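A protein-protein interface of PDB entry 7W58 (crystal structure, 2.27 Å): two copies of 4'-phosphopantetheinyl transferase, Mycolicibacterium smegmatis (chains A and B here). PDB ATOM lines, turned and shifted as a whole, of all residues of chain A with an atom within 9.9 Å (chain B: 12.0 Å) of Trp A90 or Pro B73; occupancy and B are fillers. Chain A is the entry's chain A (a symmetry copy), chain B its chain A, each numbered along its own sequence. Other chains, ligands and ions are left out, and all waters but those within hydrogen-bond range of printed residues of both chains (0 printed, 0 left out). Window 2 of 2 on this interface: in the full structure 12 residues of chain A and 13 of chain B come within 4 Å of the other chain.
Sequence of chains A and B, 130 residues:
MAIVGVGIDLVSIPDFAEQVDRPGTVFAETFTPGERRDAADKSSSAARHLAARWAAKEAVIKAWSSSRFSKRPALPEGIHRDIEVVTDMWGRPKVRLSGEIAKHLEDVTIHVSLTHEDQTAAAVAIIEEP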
ATOM      1  N   HIS A  49      23.490  20.751 -17.967  1.00  0.00           N
ATOM      2  CA  HIS A  49      23.293  20.012 -16.725  1.00  0.00           C
ATOM      3  C   HIS A  49      23.878  18.606 -16.790  1.00  0.00           C
ATOM      4  O   HIS A  49      24.354  18.087 -15.781  1.00  0.00           O
ATOM      5  CB  HIS A  49      21.819  19.990 -16.286  1.00  0.00           C
ATOM      6  CG  HIS A  49      21.332  21.345 -15.905  1.00  0.00           C
ATOM      7  ND1 HIS A  49      20.280  21.958 -16.550  1.00  0.00           N
ATOM      8  CD2 HIS A  49      21.797  22.229 -14.995  1.00  0.00           C
ATOM      9  CE1 HIS A  49      20.101  23.161 -16.042  1.00  0.00           C
ATOM     10  NE2 HIS A  49      21.019  23.349 -15.080  1.00  0.00           N
ATOM     11  N   VAL A  86      23.665  11.812  -9.100  1.00  0.00           N
ATOM     12  CA  VAL A  86      22.351  12.299  -9.473  1.00  0.00           C
ATOM     13  C   VAL A  86      22.173  13.699  -8.889  1.00  0.00           C
ATOM     14  O   VAL A  86      22.935  14.102  -8.013  1.00  0.00           O
ATOM     15  CB  VAL A  86      21.239  11.327  -9.025  1.00  0.00           C
ATOM     16  CG1 VAL A  86      21.358   9.980  -9.723  1.00  0.00           C
ATOM     17  CG2 VAL A  86      21.204  11.147  -7.514  1.00  0.00           C
ATOM     18  N   THR A  87      21.169  14.425  -9.401  1.00  0.00           N
ATOM     19  CA  THR A  87      20.815  15.749  -8.915  1.00  0.00           C
ATOM     20  C   THR A  87      19.373  15.760  -8.414  1.00  0.00           C
ATOM     21  O   THR A  87      18.503  15.110  -8.983  1.00  0.00           O
ATOM     22  CB  THR A  87      21.032  16.808 -10.002  1.00  0.00           C
ATOM     23  OG1 THR A  87      20.436  16.311 -11.202  1.00  0.00           O
ATOM     24  CG2 THR A  87      22.496  17.109 -10.239  1.00  0.00           C
ATOM     25  N   ASP A  88      19.131  16.504  -7.328  1.00  0.00           N
ATOM     26  CA  ASP A  88      17.777  16.733  -6.845  1.00  0.00           C
ATOM     27  C   ASP A  88      17.131  17.825  -7.700  1.00  0.00           C
ATOM     28  O   ASP A  88      17.777  18.382  -8.588  1.00  0.00           O
ATOM     29  CB  ASP A  88      17.744  16.950  -5.324  1.00  0.00           C
ATOM     30  CG  ASP A  88      18.377  18.239  -4.818  1.00  0.00           C
ATOM     31  OD1 ASP A  88      18.709  19.117  -5.646  1.00  0.00           O
ATOM     32  OD2 ASP A  88      18.522  18.367  -3.581  1.00  0.00           O
ATOM     33  N   MET A  89      15.859  18.141  -7.417  1.00  0.00           N
ATOM     34  CA  MET A  89      15.128  19.098  -8.236  1.00  0.00           C
ATOM     35  C   MET A  89      15.603  20.529  -7.981  1.00  0.00           C
ATOM     36  O   MET A  89      15.102  21.465  -8.596  1.00  0.00           O
ATOM     37  CB  MET A  89      13.606  18.984  -8.087  1.00  0.00           C
ATOM     38  CG  MET A  89      13.138  18.107  -6.941  1.00  0.00           C
ATOM     39  SD  MET A  89      11.438  17.518  -7.203  1.00  0.00           S
ATOM     40  CE  MET A  89      11.708  16.225  -8.418  1.00  0.00           C
ATOM     41  N   TRP A  90      16.601  20.694  -7.107  1.00  0.00           N
ATOM     42  CA  TRP A  90      17.235  21.992  -6.944  1.00  0.00           C
ATOM     43  C   TRP A  90      18.636  21.978  -7.547  1.00  0.00           C
ATOM     44  O   TRP A  90      19.368  22.959  -7.437  1.00  0.00           O
ATOM     45  CB  TRP A  90      17.239  22.425  -5.474  1.00  0.00           C
ATOM     46  CG  TRP A  90      15.861  22.471  -4.895  1.00  0.00           C
ATOM     47  CD1 TRP A  90      15.042  23.561  -4.791  1.00  0.00           C
ATOM     48  CD2 TRP A  90      15.119  21.356  -4.370  1.00  0.00           C
ATOM     49  NE1 TRP A  90      13.850  23.205  -4.221  1.00  0.00           N
ATOM     50  CE2 TRP A  90      13.867  21.858  -3.954  1.00  0.00           C
ATOM     51  CE3 TRP A  90      15.392  19.993  -4.204  1.00  0.00           C
ATOM     52  CZ2 TRP A  90      12.896  21.035  -3.378  1.00  0.00           C
ATOM     53  CZ3 TRP A  90      14.431  19.181  -3.638  1.00  0.00           C
ATOM     54  CH2 TRP A  90      13.200  19.699  -3.231  1.00  0.00           C
ATOM     55  N   GLY A  91      18.988  20.852  -8.182  1.00  0.00           N
ATOM     56  CA  GLY A  91      20.264  20.693  -8.863  1.00  0.00           C
ATOM     57  C   GLY A  91      21.429  20.401  -7.917  1.00  0.00           C
ATOM     58  O   GLY A  91      22.582  20.612  -8.286  1.00  0.00           O
ATOM     59  N   ARG A  92      21.130  19.924  -6.700  1.00  0.00           N
ATOM     60  CA  ARG A  92      22.170  19.548  -5.749  1.00  0.00           C
ATOM     61  C   ARG A  92      22.560  18.091  -5.983  1.00  0.00           C
ATOM     62  O   ARG A  92      21.703  17.208  -6.010  1.00  0.00           O
ATOM     63  CB  ARG A  92      21.749  19.805  -4.296  1.00  0.00           C
ATOM     64  CG  ARG A  92      21.632  21.281  -3.929  1.00  0.00           C
ATOM     65  CD  ARG A  92      21.084  21.560  -2.535  1.00  0.00           C
ATOM     66  NE  ARG A  92      19.881  20.790  -2.228  1.00  0.00           N
ATOM     67  CZ  ARG A  92      19.147  20.903  -1.123  1.00  0.00           C
ATOM     68  NH1 ARG A  92      19.478  21.778  -0.186  1.00  0.00           N
ATOM     69  NH2 ARG A  92      18.079  20.139  -0.965  1.00  0.00           N
ATOM     70  N   PRO A  93      23.868  17.804  -6.183  1.00  0.00           N
ATOM     71  CA  PRO A  93      24.322  16.455  -6.507  1.00  0.00           C
ATOM     72  C   PRO A  93      24.323  15.517  -5.301  1.00  0.00           C
ATOM     73  O   PRO A  93      24.428  15.947  -4.155  1.00  0.00           O
ATOM     74  CB  PRO A  93      25.750  16.695  -7.012  1.00  0.00           C
ATOM     75  CG  PRO A  93      26.204  17.885  -6.212  1.00  0.00           C
ATOM     76  CD  PRO A  93      24.976  18.767  -6.121  1.00  0.00           C
ATOM     77  N   LYS A  94      24.216  14.227  -5.603  1.00  0.00           N
ATOM     78  CA  LYS A  94      24.146  13.163  -4.624  1.00  0.00           C
ATOM     79  C   LYS A  94      24.893  11.970  -5.218  1.00  0.00           C
ATOM     80  O   LYS A  94      24.670  11.622  -6.382  1.00  0.00           O
ATOM     81  CB  LYS A  94      22.668  12.821  -4.396  1.00  0.00           C
ATOM     82  CG  LYS A  94      22.195  12.789  -2.946  1.00  0.00           C
ATOM     83  CD  LYS A  94      22.041  14.148  -2.286  1.00  0.00           C
ATOM     84  CE  LYS A  94      21.408  14.056  -0.910  1.00  0.00           C
ATOM     85  NZ  LYS A  94      22.327  13.504   0.124  1.00  0.00           N
ATOM     86  N   LEU A 114      29.019  20.718  -7.937  1.00  0.00           N
ATOM     87  CA  LEU A 114      29.074  20.945  -9.373  1.00  0.00           C
ATOM     88  C   LEU A 114      28.507  22.327  -9.705  1.00  0.00           C
ATOM     89  O   LEU A 114      27.786  22.924  -8.916  1.00  0.00           O
ATOM     90  CB  LEU A 114      28.354  19.828 -10.153  1.00  0.00           C
ATOM     91  CG  LEU A 114      26.933  19.440  -9.711  1.00  0.00           C
ATOM     92  CD1 LEU A 114      25.914  20.542  -9.986  1.00  0.00           C
ATOM     93  CD2 LEU A 114      26.495  18.160 -10.399  1.00  0.00           C
ATOM     94  N   HIS A 116      28.103  25.172 -13.540  1.00  0.00           N
ATOM     95  CA  HIS A 116      28.321  25.382 -14.959  1.00  0.00           C
ATOM     96  C   HIS A 116      28.039  26.839 -15.290  1.00  0.00           C
ATOM     97  O   HIS A 116      27.275  27.495 -14.587  1.00  0.00           O
ATOM     98  CB  HIS A 116      27.425  24.449 -15.788  1.00  0.00           C
ATOM     99  CG  HIS A 116      25.998  24.885 -15.809  1.00  0.00           C
ATOM    100  ND1 HIS A 116      25.552  25.909 -16.634  1.00  0.00           N
ATOM    101  CD2 HIS A 116      24.928  24.468 -15.103  1.00  0.00           C
ATOM    102  CE1 HIS A 116      24.267  26.103 -16.439  1.00  0.00           C
ATOM    103  NE2 HIS A 116      23.858  25.226 -15.508  1.00  0.00           N
ATOM    104  N   ILE B   8      31.562  24.683  -5.042  1.00  0.00           N
ATOM    105  CA  ILE B   8      32.331  25.242  -6.139  1.00  0.00           C
ATOM    106  C   ILE B   8      31.373  26.075  -6.995  1.00  0.00           C
ATOM    107  O   ILE B   8      30.177  25.789  -7.051  1.00  0.00           O
ATOM    108  CB  ILE B   8      33.089  24.132  -6.904  1.00  0.00           C
ATOM    109  CG1 ILE B   8      34.054  24.694  -7.956  1.00  0.00           C
ATOM    110  CG2 ILE B   8      32.134  23.091  -7.487  1.00  0.00           C
ATOM    111  CD1 ILE B   8      34.952  23.653  -8.595  1.00  0.00           C
ATOM    112  N   ASP B   9      31.877  27.165  -7.584  1.00  0.00           N
ATOM    113  CA  ASP B   9      31.055  27.979  -8.465  1.00  0.00           C
ATOM    114  C   ASP B   9      31.889  28.531  -9.618  1.00  0.00           C
ATOM    115  O   ASP B   9      33.011  28.990  -9.418  1.00  0.00           O
ATOM    116  CB  ASP B   9      30.324  29.097  -7.719  1.00  0.00           C
ATOM    117  CG  ASP B   9      29.196  29.681  -8.555  1.00  0.00           C
ATOM    118  OD1 ASP B   9      28.380  28.895  -9.070  1.00  0.00           O
ATOM    119  OD2 ASP B   9      29.167  30.907  -8.727  1.00  0.00           O
ATOM    120  N   GLU B  58      28.849  32.612  -3.727  1.00  0.00           N
ATOM    121  CA  GLU B  58      28.064  31.482  -4.210  1.00  0.00           C
ATOM    122  C   GLU B  58      28.631  30.160  -3.696  1.00  0.00           C
ATOM    123  O   GLU B  58      27.885  29.326  -3.176  1.00  0.00           O
ATOM    124  CB  GLU B  58      28.012  31.458  -5.736  1.00  0.00           C
ATOM    125  CG  GLU B  58      27.189  32.581  -6.331  1.00  0.00           C
ATOM    126  CD  GLU B  58      25.688  32.386  -6.223  1.00  0.00           C
ATOM    127  OE1 GLU B  58      25.093  31.877  -7.192  1.00  0.00           O
ATOM    128  OE2 GLU B  58      25.119  32.754  -5.180  1.00  0.00           O
ATOM    129  N   ILE B  61      27.755  29.763  -0.110  1.00  0.00           N
ATOM    130  CA  ILE B  61      26.336  29.498   0.071  1.00  0.00           C
ATOM    131  C   ILE B  61      26.005  28.048  -0.289  1.00  0.00           C
ATOM    132  O   ILE B  61      25.192  27.423   0.394  1.00  0.00           O
ATOM    133  CB  ILE B  61      25.484  30.515  -0.717  1.00  0.00           C
ATOM    134  CG1 ILE B  61      25.512  31.891  -0.048  1.00  0.00           C
ATOM    135  CG2 ILE B  61      24.060  30.005  -0.912  1.00  0.00           C
ATOM    136  CD1 ILE B  61      24.995  33.006  -0.928  1.00  0.00           C
ATOM    137  N   LYS B  62      26.636  27.513  -1.345  1.00  0.00           N
ATOM    138  CA  LYS B  62      26.426  26.127  -1.756  1.00  0.00           C
ATOM    139  C   LYS B  62      26.880  25.163  -0.656  1.00  0.00           C
ATOM    140  O   LYS B  62      26.159  24.224  -0.318  1.00  0.00           O
ATOM    141  CB  LYS B  62      27.088  25.834  -3.108  1.00  0.00           C
ATOM    142  CG  LYS B  62      26.183  26.024  -4.320  1.00  0.00           C
ATOM    143  CD  LYS B  62      26.905  26.406  -5.602  1.00  0.00           C
ATOM    144  CE  LYS B  62      26.899  25.352  -6.690  1.00  0.00           C
ATOM    145  NZ  LYS B  62      27.262  25.941  -8.008  1.00  0.00           N
ATOM    146  N   ALA B  63      28.069  25.418  -0.090  1.00  0.00           N
ATOM    147  CA  ALA B  63      28.604  24.626   1.010  1.00  0.00           C
ATOM    148  C   ALA B  63      27.635  24.654   2.190  1.00  0.00           C
ATOM    149  O   ALA B  63      27.473  23.653   2.881  1.00  0.00           O
ATOM    150  CB  ALA B  63      29.979  25.123   1.409  1.00  0.00           C
ATOM    151  N   TRP B  64      26.994  25.809   2.401  1.00  0.00           N
ATOM    152  CA  TRP B  64      26.057  25.987   3.497  1.00  0.00           C
ATOM    153  C   TRP B  64      24.768  25.209   3.226  1.00  0.00           C
ATOM    154  O   TRP B  64      24.275  24.510   4.105  1.00  0.00           O
ATOM    155  CB  TRP B  64      25.797  27.478   3.736  1.00  0.00           C
ATOM    156  CG  TRP B  64      24.833  27.708   4.856  1.00  0.00           C
ATOM    157  CD1 TRP B  64      25.143  27.889   6.172  1.00  0.00           C
ATOM    158  CD2 TRP B  64      23.396  27.749   4.763  1.00  0.00           C
ATOM    159  NE1 TRP B  64      23.998  28.029   6.904  1.00  0.00           N
ATOM    160  CE2 TRP B  64      22.910  27.952   6.071  1.00  0.00           C
ATOM    161  CE3 TRP B  64      22.476  27.630   3.715  1.00  0.00           C
ATOM    162  CZ2 TRP B  64      21.544  28.054   6.350  1.00  0.00           C
ATOM    163  CZ3 TRP B  64      21.128  27.707   3.989  1.00  0.00           C
ATOM    164  CH2 TRP B  64      20.670  27.928   5.292  1.00  0.00           C
ATOM    165  N   SER B  65      24.246  25.346   2.001  1.00  0.00           N
ATOM    166  CA  SER B  65      23.052  24.672   1.509  1.00  0.00           C
ATOM    167  C   SER B  65      23.111  23.162   1.673  1.00  0.00           C
ATOM    168  O   SER B  65      22.079  22.549   1.919  1.00  0.00           O
ATOM    169  CB  SER B  65      22.832  24.969   0.068  1.00  0.00           C
ATOM    170  OG  SER B  65      22.124  26.171  -0.048  1.00  0.00           O
ATOM    171  N   SER B  66      24.293  22.582   1.448  1.00  0.00           N
ATOM    172  CA  SER B  66      24.473  21.136   1.432  1.00  0.00           C
ATOM    173  C   SER B  66      24.731  20.613   2.843  1.00  0.00           C
ATOM    174  O   SER B  66      24.787  19.399   3.048  1.00  0.00           O
ATOM    175  CB  SER B  66      25.622  20.754   0.524  1.00  0.00           C
ATOM    176  OG  SER B  66      26.878  21.029   1.161  1.00  0.00           O
ATOM    177  N   SER B  67      24.917  21.543   3.793  1.00  0.00           N
ATOM    178  CA  SER B  67      25.286  21.229   5.163  1.00  0.00           C
ATOM    179  C   SER B  67      24.046  21.042   6.036  1.00  0.00           C
ATOM    180  O   SER B  67      22.924  21.289   5.602  1.00  0.00           O
ATOM    181  CB  SER B  67      26.167  22.301   5.736  1.00  0.00           C
ATOM    182  OG  SER B  67      25.376  23.330   6.309  1.00  0.00           O
ATOM    183  N   ARG B  68      24.289  20.652   7.289  1.00  0.00           N
ATOM    184  CA  ARG B  68      23.261  20.391   8.281  1.00  0.00           C
ATOM    185  C   ARG B  68      22.699  21.696   8.850  1.00  0.00           C
ATOM    186  O   ARG B  68      21.776  21.672   9.666  1.00  0.00           O
ATOM    187  CB  ARG B  68      23.848  19.536   9.408  1.00  0.00           C
ATOM    188  CG  ARG B  68      24.857  20.266  10.283  1.00  0.00           C
ATOM    189  CD  ARG B  68      25.248  19.493  11.534  1.00  0.00           C
ATOM    190  NE  ARG B  68      26.240  20.230  12.308  1.00  0.00           N
ATOM    191  CZ  ARG B  68      27.550  20.009  12.268  1.00  0.00           C
ATOM    192  NH1 ARG B  68      28.053  19.056  11.502  1.00  0.00           N
ATOM    193  NH2 ARG B  68      28.354  20.749  13.009  1.00  0.00           N
ATOM    194  N   PHE B  69      23.266  22.834   8.436  1.00  0.00           N
ATOM    195  CA  PHE B  69      22.821  24.121   8.948  1.00  0.00           C
ATOM    196  C   PHE B  69      21.635  24.619   8.134  1.00  0.00           C
ATOM    197  O   PHE B  69      20.982  25.582   8.531  1.00  0.00           O
ATOM    198  CB  PHE B  69      23.953  25.148   8.940  1.00  0.00           C
ATOM    199  CG  PHE B  69      25.032  24.854   9.946  1.00  0.00           C
ATOM    200  CD1 PHE B  69      24.789  24.993  11.306  1.00  0.00           C
ATOM    201  CD2 PHE B  69      26.281  24.419   9.538  1.00  0.00           C
ATOM    202  CE1 PHE B  69      25.780  24.721  12.238  1.00  0.00           C
ATOM    203  CE2 PHE B  69      27.270  24.141  10.472  1.00  0.00           C
ATOM    204  CZ  PHE B  69      27.021  24.301  11.819  1.00  0.00           C
ATOM    205  N   SER B  70      21.392  23.945   7.003  1.00  0.00           N
ATOM    206  CA  SER B  70      20.270  24.221   6.123  1.00  0.00           C
ATOM    207  C   SER B  70      19.150  23.214   6.388  1.00  0.00           C
ATOM    208  O   SER B  70      19.377  22.001   6.362  1.00  0.00           O
ATOM    209  CB  SER B  70      20.718  24.184   4.682  1.00  0.00           C
ATOM    210  OG  SER B  70      19.633  24.447   3.810  1.00  0.00           O
ATOM    211  N   LYS B  71      17.944  23.732   6.643  1.00  0.00           N
ATOM    212  CA  LYS B  71      16.789  22.894   6.936  1.00  0.00           C
ATOM    213  C   LYS B  71      15.924  22.735   5.685  1.00  0.00           C
ATOM    214  O   LYS B  71      15.838  21.635   5.140  1.00  0.00           O
ATOM    215  CB  LYS B  71      16.028  23.426   8.155  1.00  0.00           C
ATOM    216  CG  LYS B  71      16.538  22.929   9.504  1.00  0.00           C
ATOM    217  CD  LYS B  71      17.822  23.582   9.982  1.00  0.00           C
ATOM    218  CE  LYS B  71      18.382  22.941  11.235  1.00  0.00           C
ATOM    219  NZ  LYS B  71      19.501  23.731  11.808  1.00  0.00           N
ATOM    220  N   ARG B  72      15.310  23.840   5.234  1.00  0.00           N
ATOM    221  CA  ARG B  72      14.516  23.856   4.011  1.00  0.00           C
ATOM    222  C   ARG B  72      15.451  23.891   2.801  1.00  0.00           C
ATOM    223  O   ARG B  72      16.555  24.426   2.886  1.00  0.00           O
ATOM    224  CB  ARG B  72      13.548  25.044   4.018  1.00  0.00           C
ATOM    225  N   PRO B  73      15.058  23.310   1.641  1.00  0.00           N
ATOM    226  CA  PRO B  73      15.886  23.356   0.432  1.00  0.00           C
ATOM    227  C   PRO B  73      16.071  24.760  -0.145  1.00  0.00           C
ATOM    228  O   PRO B  73      17.081  25.028  -0.797  1.00  0.00           O
ATOM    229  CB  PRO B  73      15.137  22.478  -0.584  1.00  0.00           C
ATOM    230  CG  PRO B  73      14.156  21.667   0.250  1.00  0.00           C
ATOM    231  CD  PRO B  73      13.821  22.538   1.442  1.00  0.00           C
ATOM    232  N   ALA B  74      15.085  25.636   0.099  1.00  0.00           N
ATOM    233  CA  ALA B  74      15.105  27.024  -0.341  1.00  0.00           C
ATOM    234  C   ALA B  74      15.913  27.876   0.641  1.00  0.00           C
ATOM    235  O   ALA B  74      15.701  27.797   1.848  1.00  0.00           O
ATOM    236  CB  ALA B  74      13.689  27.528  -0.466  1.00  0.00           C
ATOM    237  N   LEU B  75      16.829  28.697   0.108  1.00  0.00           N
ATOM    238  CA  LEU B  75      17.734  29.511   0.910  1.00  0.00           C
ATOM    239  C   LEU B  75      16.910  30.392   1.845  1.00  0.00           C
ATOM    240  O   LEU B  75      15.789  30.756   1.504  1.00  0.00           O
ATOM    241  CB  LEU B  75      18.605  30.370  -0.015  1.00  0.00           C
ATOM    242  CG  LEU B  75      19.491  29.634  -1.025  1.00  0.00           C
ATOM    243  CD1 LEU B  75      20.277  30.621  -1.876  1.00  0.00           C
ATOM    244  CD2 LEU B  75      20.449  28.685  -0.331  1.00  0.00           C
ATOM    245  N   PRO B  76      17.411  30.757   3.049  1.00  0.00           N
ATOM    246  CA  PRO B  76      16.665  31.638   3.950  1.00  0.00           C
ATOM    247  C   PRO B  76      16.715  33.103   3.516  1.00  0.00           C
ATOM    248  O   PRO B  76      17.411  33.456   2.563  1.00  0.00           O
ATOM    249  CB  PRO B  76      17.351  31.420   5.309  1.00  0.00           C
ATOM    250  CG  PRO B  76      18.777  31.059   4.954  1.00  0.00           C
ATOM    251  CD  PRO B  76      18.698  30.334   3.622  1.00  0.00           C
ATOM    252  N   GLU B  77      15.954  33.942   4.229  1.00  0.00           N
ATOM    253  CA  GLU B  77      15.871  35.367   3.961  1.00  0.00           C
ATOM    254  C   GLU B  77      17.211  36.019   4.295  1.00  0.00           C
ATOM    255  O   GLU B  77      17.739  35.836   5.393  1.00  0.00           O
ATOM    256  CB  GLU B  77      14.710  35.978   4.758  1.00  0.00           C
ATOM    257  CG  GLU B  77      14.670  37.500   4.765  1.00  0.00           C
ATOM    258  CD  GLU B  77      14.348  38.159   3.432  1.00  0.00           C
ATOM    259  OE1 GLU B  77      13.314  37.798   2.830  1.00  0.00           O
ATOM    260  OE2 GLU B  77      15.136  39.028   2.995  1.00  0.00           O
ATOM    261  N   ILE B  79      20.273  35.628   3.336  1.00  0.00           N
ATOM    262  CA  ILE B  79      21.516  34.877   3.296  1.00  0.00           C
ATOM    263  C   ILE B  79      22.572  35.735   2.600  1.00  0.00           C
ATOM    264  O   ILE B  79      23.756  35.666   2.921  1.00  0.00           O
ATOM    265  CB  ILE B  79      21.286  33.522   2.587  1.00  0.00           C
ATOM    266  CG1 ILE B  79      22.502  32.593   2.662  1.00  0.00           C
ATOM    267  CG2 ILE B  79      20.792  33.714   1.161  1.00  0.00           C
ATOM    268  CD1 ILE B  79      22.411  31.565   3.760  1.00  0.00           C
ATOM    269  N   HIS B  80      22.111  36.593   1.682  1.00  0.00           N
ATOM    270  CA  HIS B  80      22.996  37.336   0.807  1.00  0.00           C
ATOM    271  C   HIS B  80      23.559  38.578   1.489  1.00  0.00           C
ATOM    272  O   HIS B  80      24.523  39.151   0.995  1.00  0.00           O
ATOM    273  CB  HIS B  80      22.309  37.621  -0.528  1.00  0.00           C
ATOM    274  CG  HIS B  80      22.346  36.438  -1.432  1.00  0.00           C
ATOM    275  ND1 HIS B  80      21.269  35.584  -1.571  1.00  0.00           N
ATOM    276  CD2 HIS B  80      23.329  35.954  -2.223  1.00  0.00           C
ATOM    277  CE1 HIS B  80      21.586  34.623  -2.417  1.00  0.00           C
ATOM    278  NE2 HIS B  80      22.846  34.830  -2.833  1.00  0.00           N
ATOM    279  N   ILE B 101      23.175  33.692  10.309  1.00  0.00           N
ATOM    280  CA  ILE B 101      24.263  32.847   9.847  1.00  0.00           C
ATOM    281  C   ILE B 101      25.443  32.971  10.814  1.00  0.00           C
ATOM    282  O   ILE B 101      25.998  31.959  11.242  1.00  0.00           O
ATOM    283  CB  ILE B 101      24.643  33.133   8.378  1.00  0.00           C
ATOM    284  CG1 ILE B 101      23.437  33.028   7.442  1.00  0.00           C
ATOM    285  CG2 ILE B 101      25.761  32.212   7.921  1.00  0.00           C
ATOM    286  CD1 ILE B 101      22.885  31.629   7.270  1.00  0.00           C
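Of the 12 printed residues of chain A, 3 touch a printed residue of chain B. Printed residues of chain B that touch a printed residue of chain A: Ile B8, Lys B62, Ser B65 and Pro B73. Hydrophobic or aromatic side chains of chain B that line the printed part of chain A: Ile B8 and Pro B73.
The side-chain amino group (NZ) of Lys B62 lies within hydrogen-bond range of the backbone carbonyl oxygen (O) of Leu A114. The guanidinium group (NH1) of Arg A92 lies within hydrogen-bond range of the backbone carbonyl oxygen (O) of Ser B65 (3.4 Å).
No position is printed for both chains.
Among the printed residues, pairs that only touch across the chains: Trp A90 with Pro B73 (3.7 Å), Arg A92 with Pro B73 (3.8 Å) and Leu A114 with Ile B8 (3.9 Å).
Of the printed residues of chain B, Trp A90 touches Pro B73. Of chain A, only Trp A90 and Arg A92 come within 4 Å of Pro B73. Asp A88 touches none of the printed residues of chain B. Arg A92 touches just these residues of chain B: Ser B65 (3.4 Å) and Pro B73 (3.8 Å). No residue of chain A comes within 4 Å of Arg B72. No residue of chain A comes within 4 Å of Ala B74. Printed residues of chain B within 4 Å of Leu A114: Ile B8 (3.9 Å) and Lys B62 (3.2 Å). Of the printed residues of chain A, Ile B8 touches Leu A114. Of the printed residues of chain A, Lys B62 touches Leu A114 (3.2 Å). Of the printed residues of chain A, Ser B65 touches Arg A92 (3.4 Å). The nearest residue of chain B that does not touch Trp A90 is Ala B74 (5.1 Å). The nearest residue of chain A that does not touch Pro B73 is Asp A88 (6.1 Å). The nearest printed residue of chain A that does not touch Ser B65 is Asp A88 (7.8 Å).
O of Ile B8 is in hydrogen-bond range of NZ of Lys B62 (3.1 Å). O of Ile B61 is in hydrogen-bond range of OG of Ser B65 (3.3 Å). OD1 of Asp B9 is in salt-bridge range of NZ of Lys B62 (3.3 Å). NE of Arg A92 is in salt-bridge range of OD2 of Asp A88 (3.1 Å). OD1 of Asp A88 lies close to N of Trp A90.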
